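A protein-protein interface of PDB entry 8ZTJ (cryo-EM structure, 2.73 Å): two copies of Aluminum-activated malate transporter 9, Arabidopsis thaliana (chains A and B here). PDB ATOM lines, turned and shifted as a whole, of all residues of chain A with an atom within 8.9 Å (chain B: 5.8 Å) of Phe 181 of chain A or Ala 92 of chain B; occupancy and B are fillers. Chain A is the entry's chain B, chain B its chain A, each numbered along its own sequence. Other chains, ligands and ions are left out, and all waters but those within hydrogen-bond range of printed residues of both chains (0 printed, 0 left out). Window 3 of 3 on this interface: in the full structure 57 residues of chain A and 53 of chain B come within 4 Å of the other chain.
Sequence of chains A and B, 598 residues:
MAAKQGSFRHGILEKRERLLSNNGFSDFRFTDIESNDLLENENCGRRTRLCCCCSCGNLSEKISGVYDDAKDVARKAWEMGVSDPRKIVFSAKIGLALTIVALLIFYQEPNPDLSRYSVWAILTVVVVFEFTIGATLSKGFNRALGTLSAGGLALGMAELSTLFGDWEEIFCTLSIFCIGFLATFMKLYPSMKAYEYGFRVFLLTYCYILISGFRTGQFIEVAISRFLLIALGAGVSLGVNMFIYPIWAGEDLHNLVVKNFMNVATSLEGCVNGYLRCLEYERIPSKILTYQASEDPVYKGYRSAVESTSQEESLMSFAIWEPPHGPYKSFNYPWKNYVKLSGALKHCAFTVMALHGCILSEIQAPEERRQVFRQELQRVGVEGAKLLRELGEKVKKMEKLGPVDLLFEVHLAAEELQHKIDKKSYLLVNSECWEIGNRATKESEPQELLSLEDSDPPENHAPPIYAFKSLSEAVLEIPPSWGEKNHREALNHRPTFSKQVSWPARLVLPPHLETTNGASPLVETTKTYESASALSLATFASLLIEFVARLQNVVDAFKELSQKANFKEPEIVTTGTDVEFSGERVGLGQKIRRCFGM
Among the printed residues, merely in contact across the chains: Thr 184 of chain A with Ile 94 of chain B, Phe 177 of chain A with Gly 95 of chain B, Phe 181 of chain A with Ser 91 of chain B, Phe 185 of chain A with Ser 91 of chain B, Thr 184 of chain A with Ser 91 of chain B, Phe 181 of chain A with Ala 92 of chain B, Phe 177 of chain A with Leu 96 of chain B and Phe 181 of chain A with Ile 88 of chain B.
Of the 10 printed residues of chain B, 6 touch a printed residue of chain A.
Hydrophobic or aromatic side chains of chain B that line the printed part of chain A: Ile 94.
Of the 16 printed residues of chain A, 4 touch a printed residue of chain B.
Among the printed residues, 8 pairs touch across the chains.
Among the printed residues, no Asp or Glu carboxylate lies within 4 Å of a Lys or Arg side-chain nitrogen of the other chain.
No position is printed for both chains.
The backbone carbonyl oxygen of Gly 180 of chain A sits at hydrogen-bond distance from the side-chain hydroxyl of Thr 184 of chain A (2.5 Å).
Of the printed residues of chain B, Phe 181 of chain A touches Ile 88 (3.99 Å), Ser 91 (3.6 Å) and Ala 92 (3.8 Å).
Ala 92 of chain B touches just one residue of chain A: Phe 181.
Of chain A, only Phe 181 (3.6 Å), Thr 184 (3.7 Å) and Phe 185 (3.6 Å) come within 4 Å of Ser 91 of chain B.
Of the printed residues of chain A, Gly 95 of chain B touches Phe 177.
Of the printed residues of chain A, Leu 96 of chain B touches Phe 177 (3.97 Å).
The nearest printed residue of chain B that does not touch Phe 181 of chain A is Gly 95 of chain B (5.0 Å).
The nearest residue of chain A that does not touch Ala 92 of chain B is Phe 177 of chain A (4.03 Å).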
ATOM      1  N   LEU A 174     -21.077   3.088  15.999  1.00  0.00           N
ATOM      2  CA  LEU A 174     -22.170   2.488  15.243  1.00  0.00           C
ATOM      3  C   LEU A 174     -23.161   3.540  14.772  1.00  0.00           C
ATOM      4  O   LEU A 174     -23.691   3.446  13.657  1.00  0.00           O
ATOM      5  CB  LEU A 174     -22.880   1.439  16.098  1.00  0.00           C
ATOM      6  CG  LEU A 174     -23.086   0.046  15.505  1.00  0.00           C
ATOM      7  CD1 LEU A 174     -21.770  -0.527  15.004  1.00  0.00           C
ATOM      8  CD2 LEU A 174     -23.719  -0.874  16.537  1.00  0.00           C
ATOM      9  N   SER A 175     -23.398   4.570  15.583  1.00  0.00           N
ATOM     10  CA  SER A 175     -24.275   5.627  15.106  1.00  0.00           C
ATOM     11  C   SER A 175     -23.582   6.442  14.024  1.00  0.00           C
ATOM     12  O   SER A 175     -24.241   6.926  13.098  1.00  0.00           O
ATOM     13  CB  SER A 175     -24.710   6.523  16.266  1.00  0.00           C
ATOM     14  OG  SER A 175     -23.602   7.195  16.837  1.00  0.00           O
ATOM     15  N   ILE A 176     -22.256   6.582  14.112  1.00  0.00           N
ATOM     16  CA  ILE A 176     -21.505   7.199  13.023  1.00  0.00           C
ATOM     17  C   ILE A 176     -21.690   6.405  11.738  1.00  0.00           C
ATOM     18  O   ILE A 176     -21.942   6.973  10.667  1.00  0.00           O
ATOM     19  CB  ILE A 176     -20.017   7.328  13.398  1.00  0.00           C
ATOM     20  CG1 ILE A 176     -19.850   8.152  14.675  1.00  0.00           C
ATOM     21  CG2 ILE A 176     -19.226   7.941  12.251  1.00  0.00           C
ATOM     22  CD1 ILE A 176     -18.443   8.649  14.899  1.00  0.00           C
ATOM     23  N   PHE A 177     -21.603   5.073  11.830  1.00  0.00           N
ATOM     24  CA  PHE A 177     -21.779   4.243  10.642  1.00  0.00           C
ATOM     25  C   PHE A 177     -23.167   4.436  10.042  1.00  0.00           C
ATOM     26  O   PHE A 177     -23.316   4.646   8.831  1.00  0.00           O
ATOM     27  CB  PHE A 177     -21.546   2.771  10.987  1.00  0.00           C
ATOM     28  CG  PHE A 177     -21.855   1.827   9.858  1.00  0.00           C
ATOM     29  CD1 PHE A 177     -20.927   1.594   8.859  1.00  0.00           C
ATOM     30  CD2 PHE A 177     -23.079   1.183   9.791  1.00  0.00           C
ATOM     31  CE1 PHE A 177     -21.210   0.730   7.818  1.00  0.00           C
ATOM     32  CE2 PHE A 177     -23.368   0.321   8.751  1.00  0.00           C
ATOM     33  CZ  PHE A 177     -22.432   0.095   7.764  1.00  0.00           C
ATOM     34  N   CYS A 178     -24.199   4.368  10.887  1.00  0.00           N
ATOM     35  CA  CYS A 178     -25.569   4.464  10.391  1.00  0.00           C
ATOM     36  C   CYS A 178     -25.852   5.832   9.780  1.00  0.00           C
ATOM     37  O   CYS A 178     -26.468   5.927   8.709  1.00  0.00           O
ATOM     38  CB  CYS A 178     -26.556   4.167  11.519  1.00  0.00           C
ATOM     39  SG  CYS A 178     -26.352   2.543  12.283  1.00  0.00           S
ATOM     40  N   ILE A 179     -25.409   6.905  10.441  1.00  0.00           N
ATOM     41  CA  ILE A 179     -25.642   8.243   9.911  1.00  0.00           C
ATOM     42  C   ILE A 179     -24.900   8.444   8.597  1.00  0.00           C
ATOM     43  O   ILE A 179     -25.438   9.039   7.658  1.00  0.00           O
ATOM     44  CB  ILE A 179     -25.249   9.308  10.951  1.00  0.00           C
ATOM     45  CG1 ILE A 179     -26.225   9.296  12.128  1.00  0.00           C
ATOM     46  CG2 ILE A 179     -25.209  10.685  10.311  1.00  0.00           C
ATOM     47  CD1 ILE A 179     -27.620   8.840  11.763  1.00  0.00           C
ATOM     48  N   GLY A 180     -23.661   7.956   8.500  1.00  0.00           N
ATOM     49  CA  GLY A 180     -22.945   8.082   7.241  1.00  0.00           C
ATOM     50  C   GLY A 180     -23.621   7.328   6.112  1.00  0.00           C
ATOM     51  O   GLY A 180     -23.765   7.852   5.002  1.00  0.00           O
ATOM     52  N   PHE A 181     -24.124   6.127   6.405  1.00  0.00           N
ATOM     53  CA  PHE A 181     -24.834   5.359   5.388  1.00  0.00           C
ATOM     54  C   PHE A 181     -26.081   6.096   4.921  1.00  0.00           C
ATOM     55  O   PHE A 181     -26.322   6.231   3.715  1.00  0.00           O
ATOM     56  CB  PHE A 181     -25.197   3.976   5.932  1.00  0.00           C
ATOM     57  CG  PHE A 181     -26.038   3.156   4.995  1.00  0.00           C
ATOM     58  CD1 PHE A 181     -25.449   2.356   4.034  1.00  0.00           C
ATOM     59  CD2 PHE A 181     -27.419   3.187   5.076  1.00  0.00           C
ATOM     60  CE1 PHE A 181     -26.221   1.602   3.172  1.00  0.00           C
ATOM     61  CE2 PHE A 181     -28.196   2.438   4.216  1.00  0.00           C
ATOM     62  CZ  PHE A 181     -27.595   1.644   3.262  1.00  0.00           C
ATOM     63  N   LEU A 182     -26.881   6.599   5.864  1.00  0.00           N
ATOM     64  CA  LEU A 182     -28.151   7.205   5.478  1.00  0.00           C
ATOM     65  C   LEU A 182     -27.932   8.526   4.751  1.00  0.00           C
ATOM     66  O   LEU A 182     -28.624   8.821   3.769  1.00  0.00           O
ATOM     67  CB  LEU A 182     -29.037   7.404   6.707  1.00  0.00           C
ATOM     68  CG  LEU A 182     -29.619   6.135   7.331  1.00  0.00           C
ATOM     69  CD1 LEU A 182     -30.065   6.390   8.760  1.00  0.00           C
ATOM     70  CD2 LEU A 182     -30.772   5.615   6.489  1.00  0.00           C
ATOM     71  N   ALA A 183     -26.985   9.341   5.222  1.00  0.00           N
ATOM     72  CA  ALA A 183     -26.709  10.609   4.561  1.00  0.00           C
ATOM     73  C   ALA A 183     -26.119  10.411   3.171  1.00  0.00           C
ATOM     74  O   ALA A 183     -26.383  11.217   2.271  1.00  0.00           O
ATOM     75  CB  ALA A 183     -25.774  11.459   5.420  1.00  0.00           C
ATOM     76  N   THR A 184     -25.327   9.353   2.965  1.00  0.00           N
ATOM     77  CA  THR A 184     -24.834   9.071   1.620  1.00  0.00           C
ATOM     78  C   THR A 184     -25.932   8.526   0.713  1.00  0.00           C
ATOM     79  O   THR A 184     -25.957   8.829  -0.486  1.00  0.00           O
ATOM     80  CB  THR A 184     -23.668   8.086   1.686  1.00  0.00           C
ATOM     81  OG1 THR A 184     -22.812   8.433   2.780  1.00  0.00           O
ATOM     82  CG2 THR A 184     -22.871   8.117   0.390  1.00  0.00           C
ATOM     83  N   PHE A 185     -26.851   7.727   1.258  1.00  0.00           N
ATOM     84  CA  PHE A 185     -27.925   7.183   0.431  1.00  0.00           C
ATOM     85  C   PHE A 185     -28.943   8.247   0.035  1.00  0.00           C
ATOM     86  O   PHE A 185     -29.461   8.227  -1.088  1.00  0.00           O
ATOM     87  CB  PHE A 185     -28.616   6.031   1.158  1.00  0.00           C
ATOM     88  CG  PHE A 185     -29.462   5.174   0.263  1.00  0.00           C
ATOM     89  CD1 PHE A 185     -28.890   4.454  -0.771  1.00  0.00           C
ATOM     90  CD2 PHE A 185     -30.830   5.088   0.454  1.00  0.00           C
ATOM     91  CE1 PHE A 185     -29.667   3.667  -1.598  1.00  0.00           C
ATOM     92  CE2 PHE A 185     -31.612   4.302  -0.369  1.00  0.00           C
ATOM     93  CZ  PHE A 185     -31.029   3.590  -1.395  1.00  0.00           C
ATOM     94  N   MET A 186     -29.243   9.188   0.932  1.00  0.00           N
ATOM     95  CA  MET A 186     -30.273  10.179   0.633  1.00  0.00           C
ATOM     96  C   MET A 186     -29.828  11.220  -0.388  1.00  0.00           C
ATOM     97  O   MET A 186     -30.685  11.875  -0.990  1.00  0.00           O
ATOM     98  CB  MET A 186     -30.718  10.876   1.918  1.00  0.00           C
ATOM     99  CG  MET A 186     -32.226  10.968   2.081  1.00  0.00           C
ATOM    100  SD  MET A 186     -33.028   9.353   2.092  1.00  0.00           S
ATOM    101  CE  MET A 186     -34.573   9.733   1.268  1.00  0.00           C
ATOM    102  N   LYS A 187     -28.527  11.389  -0.605  1.00  0.00           N
ATOM    103  CA  LYS A 187     -28.033  12.401  -1.530  1.00  0.00           C
ATOM    104  C   LYS A 187     -27.852  11.890  -2.953  1.00  0.00           C
ATOM    105  O   LYS A 187     -27.568  12.694  -3.848  1.00  0.00           O
ATOM    106  CB  LYS A 187     -26.703  12.972  -1.028  1.00  0.00           C
ATOM    107  CG  LYS A 187     -25.489  12.154  -1.425  1.00  0.00           C
ATOM    108  CD  LYS A 187     -24.203  12.943  -1.247  1.00  0.00           C
ATOM    109  CE  LYS A 187     -23.088  12.374  -2.111  1.00  0.00           C
ATOM    110  NZ  LYS A 187     -21.818  12.198  -1.357  1.00  0.00           N
ATOM    111  N   LEU A 188     -28.009  10.590  -3.190  1.00  0.00           N
ATOM    112  CA  LEU A 188     -27.864  10.018  -4.523  1.00  0.00           C
ATOM    113  C   LEU A 188     -29.153  10.041  -5.335  1.00  0.00           C
ATOM    114  O   LEU A 188     -29.142   9.608  -6.491  1.00  0.00           O
ATOM    115  CB  LEU A 188     -27.350   8.578  -4.427  1.00  0.00           C
ATOM    116  CG  LEU A 188     -25.922   8.404  -3.910  1.00  0.00           C
ATOM    117  CD1 LEU A 188     -25.575   6.932  -3.776  1.00  0.00           C
ATOM    118  CD2 LEU A 188     -24.939   9.110  -4.826  1.00  0.00           C
ATOM    119  N   LEU A 203     -23.181  16.029   7.560  1.00  0.00           N
ATOM    120  CA  LEU A 203     -22.254  14.993   7.994  1.00  0.00           C
ATOM    121  C   LEU A 203     -21.052  15.591   8.713  1.00  0.00           C
ATOM    122  O   LEU A 203     -20.608  15.061   9.740  1.00  0.00           O
ATOM    123  CB  LEU A 203     -21.802  14.159   6.795  1.00  0.00           C
ATOM    124  CG  LEU A 203     -21.523  12.675   7.042  1.00  0.00           C
ATOM    125  CD1 LEU A 203     -22.567  12.071   7.969  1.00  0.00           C
ATOM    126  CD2 LEU A 203     -21.458  11.913   5.729  1.00  0.00           C
ATOM    127  N   ILE B  88     -25.986   1.171  -3.138  1.00  0.00           N
ATOM    128  CA  ILE B  88     -26.061   0.671  -1.770  1.00  0.00           C
ATOM    129  C   ILE B  88     -24.732   0.104  -1.278  1.00  0.00           C
ATOM    130  O   ILE B  88     -24.545  -0.035  -0.060  1.00  0.00           O
ATOM    131  CB  ILE B  88     -27.180  -0.387  -1.648  1.00  0.00           C
ATOM    132  CG1 ILE B  88     -27.041  -1.188  -0.354  1.00  0.00           C
ATOM    133  CG2 ILE B  88     -27.176  -1.308  -2.853  1.00  0.00           C
ATOM    134  CD1 ILE B  88     -28.318  -1.869   0.077  1.00  0.00           C
ATOM    135  N   VAL B  89     -23.797  -0.203  -2.179  1.00  0.00           N
ATOM    136  CA  VAL B  89     -22.457  -0.602  -1.764  1.00  0.00           C
ATOM    137  C   VAL B  89     -21.577   0.613  -1.484  1.00  0.00           C
ATOM    138  O   VAL B  89     -20.719   0.571  -0.595  1.00  0.00           O
ATOM    139  CB  VAL B  89     -21.824  -1.513  -2.829  1.00  0.00           C
ATOM    140  CG1 VAL B  89     -20.433  -1.948  -2.398  1.00  0.00           C
ATOM    141  CG2 VAL B  89     -22.710  -2.718  -3.089  1.00  0.00           C
ATOM    142  N   PHE B  90     -21.780   1.710  -2.218  1.00  0.00           N
ATOM    143  CA  PHE B  90     -20.965   2.906  -2.025  1.00  0.00           C
ATOM    144  C   PHE B  90     -21.196   3.521  -0.648  1.00  0.00           C
ATOM    145  O   PHE B  90     -20.240   3.920   0.033  1.00  0.00           O
ATOM    146  CB  PHE B  90     -21.280   3.908  -3.138  1.00  0.00           C
ATOM    147  CG  PHE B  90     -20.373   5.103  -3.163  1.00  0.00           C
ATOM    148  CD1 PHE B  90     -19.029   4.966  -3.457  1.00  0.00           C
ATOM    149  CD2 PHE B  90     -20.874   6.371  -2.915  1.00  0.00           C
ATOM    150  CE1 PHE B  90     -18.199   6.068  -3.486  1.00  0.00           C
ATOM    151  CE2 PHE B  90     -20.048   7.474  -2.945  1.00  0.00           C
ATOM    152  CZ  PHE B  90     -18.710   7.323  -3.230  1.00  0.00           C
ATOM    153  N   SER B  91     -22.458   3.607  -0.223  1.00  0.00           N
ATOM    154  CA  SER B  91     -22.763   4.170   1.088  1.00  0.00           C
ATOM    155  C   SER B  91     -22.171   3.321   2.204  1.00  0.00           C
ATOM    156  O   SER B  91     -21.622   3.851   3.178  1.00  0.00           O
ATOM    157  CB  SER B  91     -24.277   4.300   1.258  1.00  0.00           C
ATOM    158  OG  SER B  91     -24.868   4.914   0.128  1.00  0.00           O
ATOM    159  N   ALA B  92     -22.270   1.996   2.076  1.00  0.00           N
ATOM    160  CA  ALA B  92     -21.681   1.106   3.068  1.00  0.00           C
ATOM    161  C   ALA B  92     -20.161   1.221   3.095  1.00  0.00           C
ATOM    162  O   ALA B  92     -19.550   1.152   4.165  1.00  0.00           O
ATOM    163  CB  ALA B  92     -22.107  -0.335   2.795  1.00  0.00           C
ATOM    164  N   LYS B  93     -19.531   1.408   1.934  1.00  0.00           N
ATOM    165  CA  LYS B  93     -18.082   1.601   1.913  1.00  0.00           C
ATOM    166  C   LYS B  93     -17.679   2.899   2.608  1.00  0.00           C
ATOM    167  O   LYS B  93     -16.688   2.934   3.353  1.00  0.00           O
ATOM    168  CB  LYS B  93     -17.577   1.585   0.472  1.00  0.00           C
ATOM    169  CG  LYS B  93     -17.613   0.215  -0.179  1.00  0.00           C
ATOM    170  CD  LYS B  93     -16.555   0.086  -1.260  1.00  0.00           C
ATOM    171  CE  LYS B  93     -16.772   1.093  -2.372  1.00  0.00           C
ATOM    172  NZ  LYS B  93     -16.123   0.663  -3.638  1.00  0.00           N
ATOM    173  N   ILE B  94     -18.433   3.974   2.377  1.00  0.00           N
ATOM    174  CA  ILE B  94     -18.143   5.235   3.059  1.00  0.00           C
ATOM    175  C   ILE B  94     -18.302   5.072   4.566  1.00  0.00           C
ATOM    176  O   ILE B  94     -17.461   5.527   5.354  1.00  0.00           O
ATOM    177  CB  ILE B  94     -19.043   6.359   2.513  1.00  0.00           C
ATOM    178  CG1 ILE B  94     -18.405   7.006   1.285  1.00  0.00           C
ATOM    179  CG2 ILE B  94     -19.305   7.404   3.585  1.00  0.00           C
ATOM    180  CD1 ILE B  94     -19.406   7.523   0.285  1.00  0.00           C
ATOM    181  N   GLY B  95     -19.389   4.421   4.988  1.00  0.00           N
ATOM    182  CA  GLY B  95     -19.571   4.149   6.405  1.00  0.00           C
ATOM    183  C   GLY B  95     -18.454   3.310   6.993  1.00  0.00           C
ATOM    184  O   GLY B  95     -18.036   3.528   8.131  1.00  0.00           O
ATOM    185  N   LEU B  96     -17.947   2.345   6.223  1.00  0.00           N
ATOM    186  CA  LEU B  96     -16.858   1.500   6.701  1.00  0.00           C
ATOM    187  C   LEU B  96     -15.577   2.300   6.900  1.00  0.00           C
ATOM    188  O   LEU B  96     -14.878   2.126   7.905  1.00  0.00           O
ATOM    189  CB  LEU B  96     -16.625   0.349   5.724  1.00  0.00           C
ATOM    190  CG  LEU B  96     -15.460  -0.592   6.030  1.00  0.00           C
ATOM    191  CD1 LEU B  96     -15.827  -1.558   7.144  1.00  0.00           C
ATOM    192  CD2 LEU B  96     -15.042  -1.344   4.778  1.00  0.00           C
ATOM    193  N   ALA B  97     -15.253   3.180   5.952  1.00  0.00           N
ATOM    194  CA  ALA B  97     -14.065   4.013   6.116  1.00  0.00           C
ATOM    195  C   ALA B  97     -14.205   4.943   7.317  1.00  0.00           C
ATOM    196  O   ALA B  97     -13.260   5.113   8.104  1.00  0.00           O
ATOM    197  CB  ALA B  97     -13.803   4.813   4.840  1.00  0.00           C
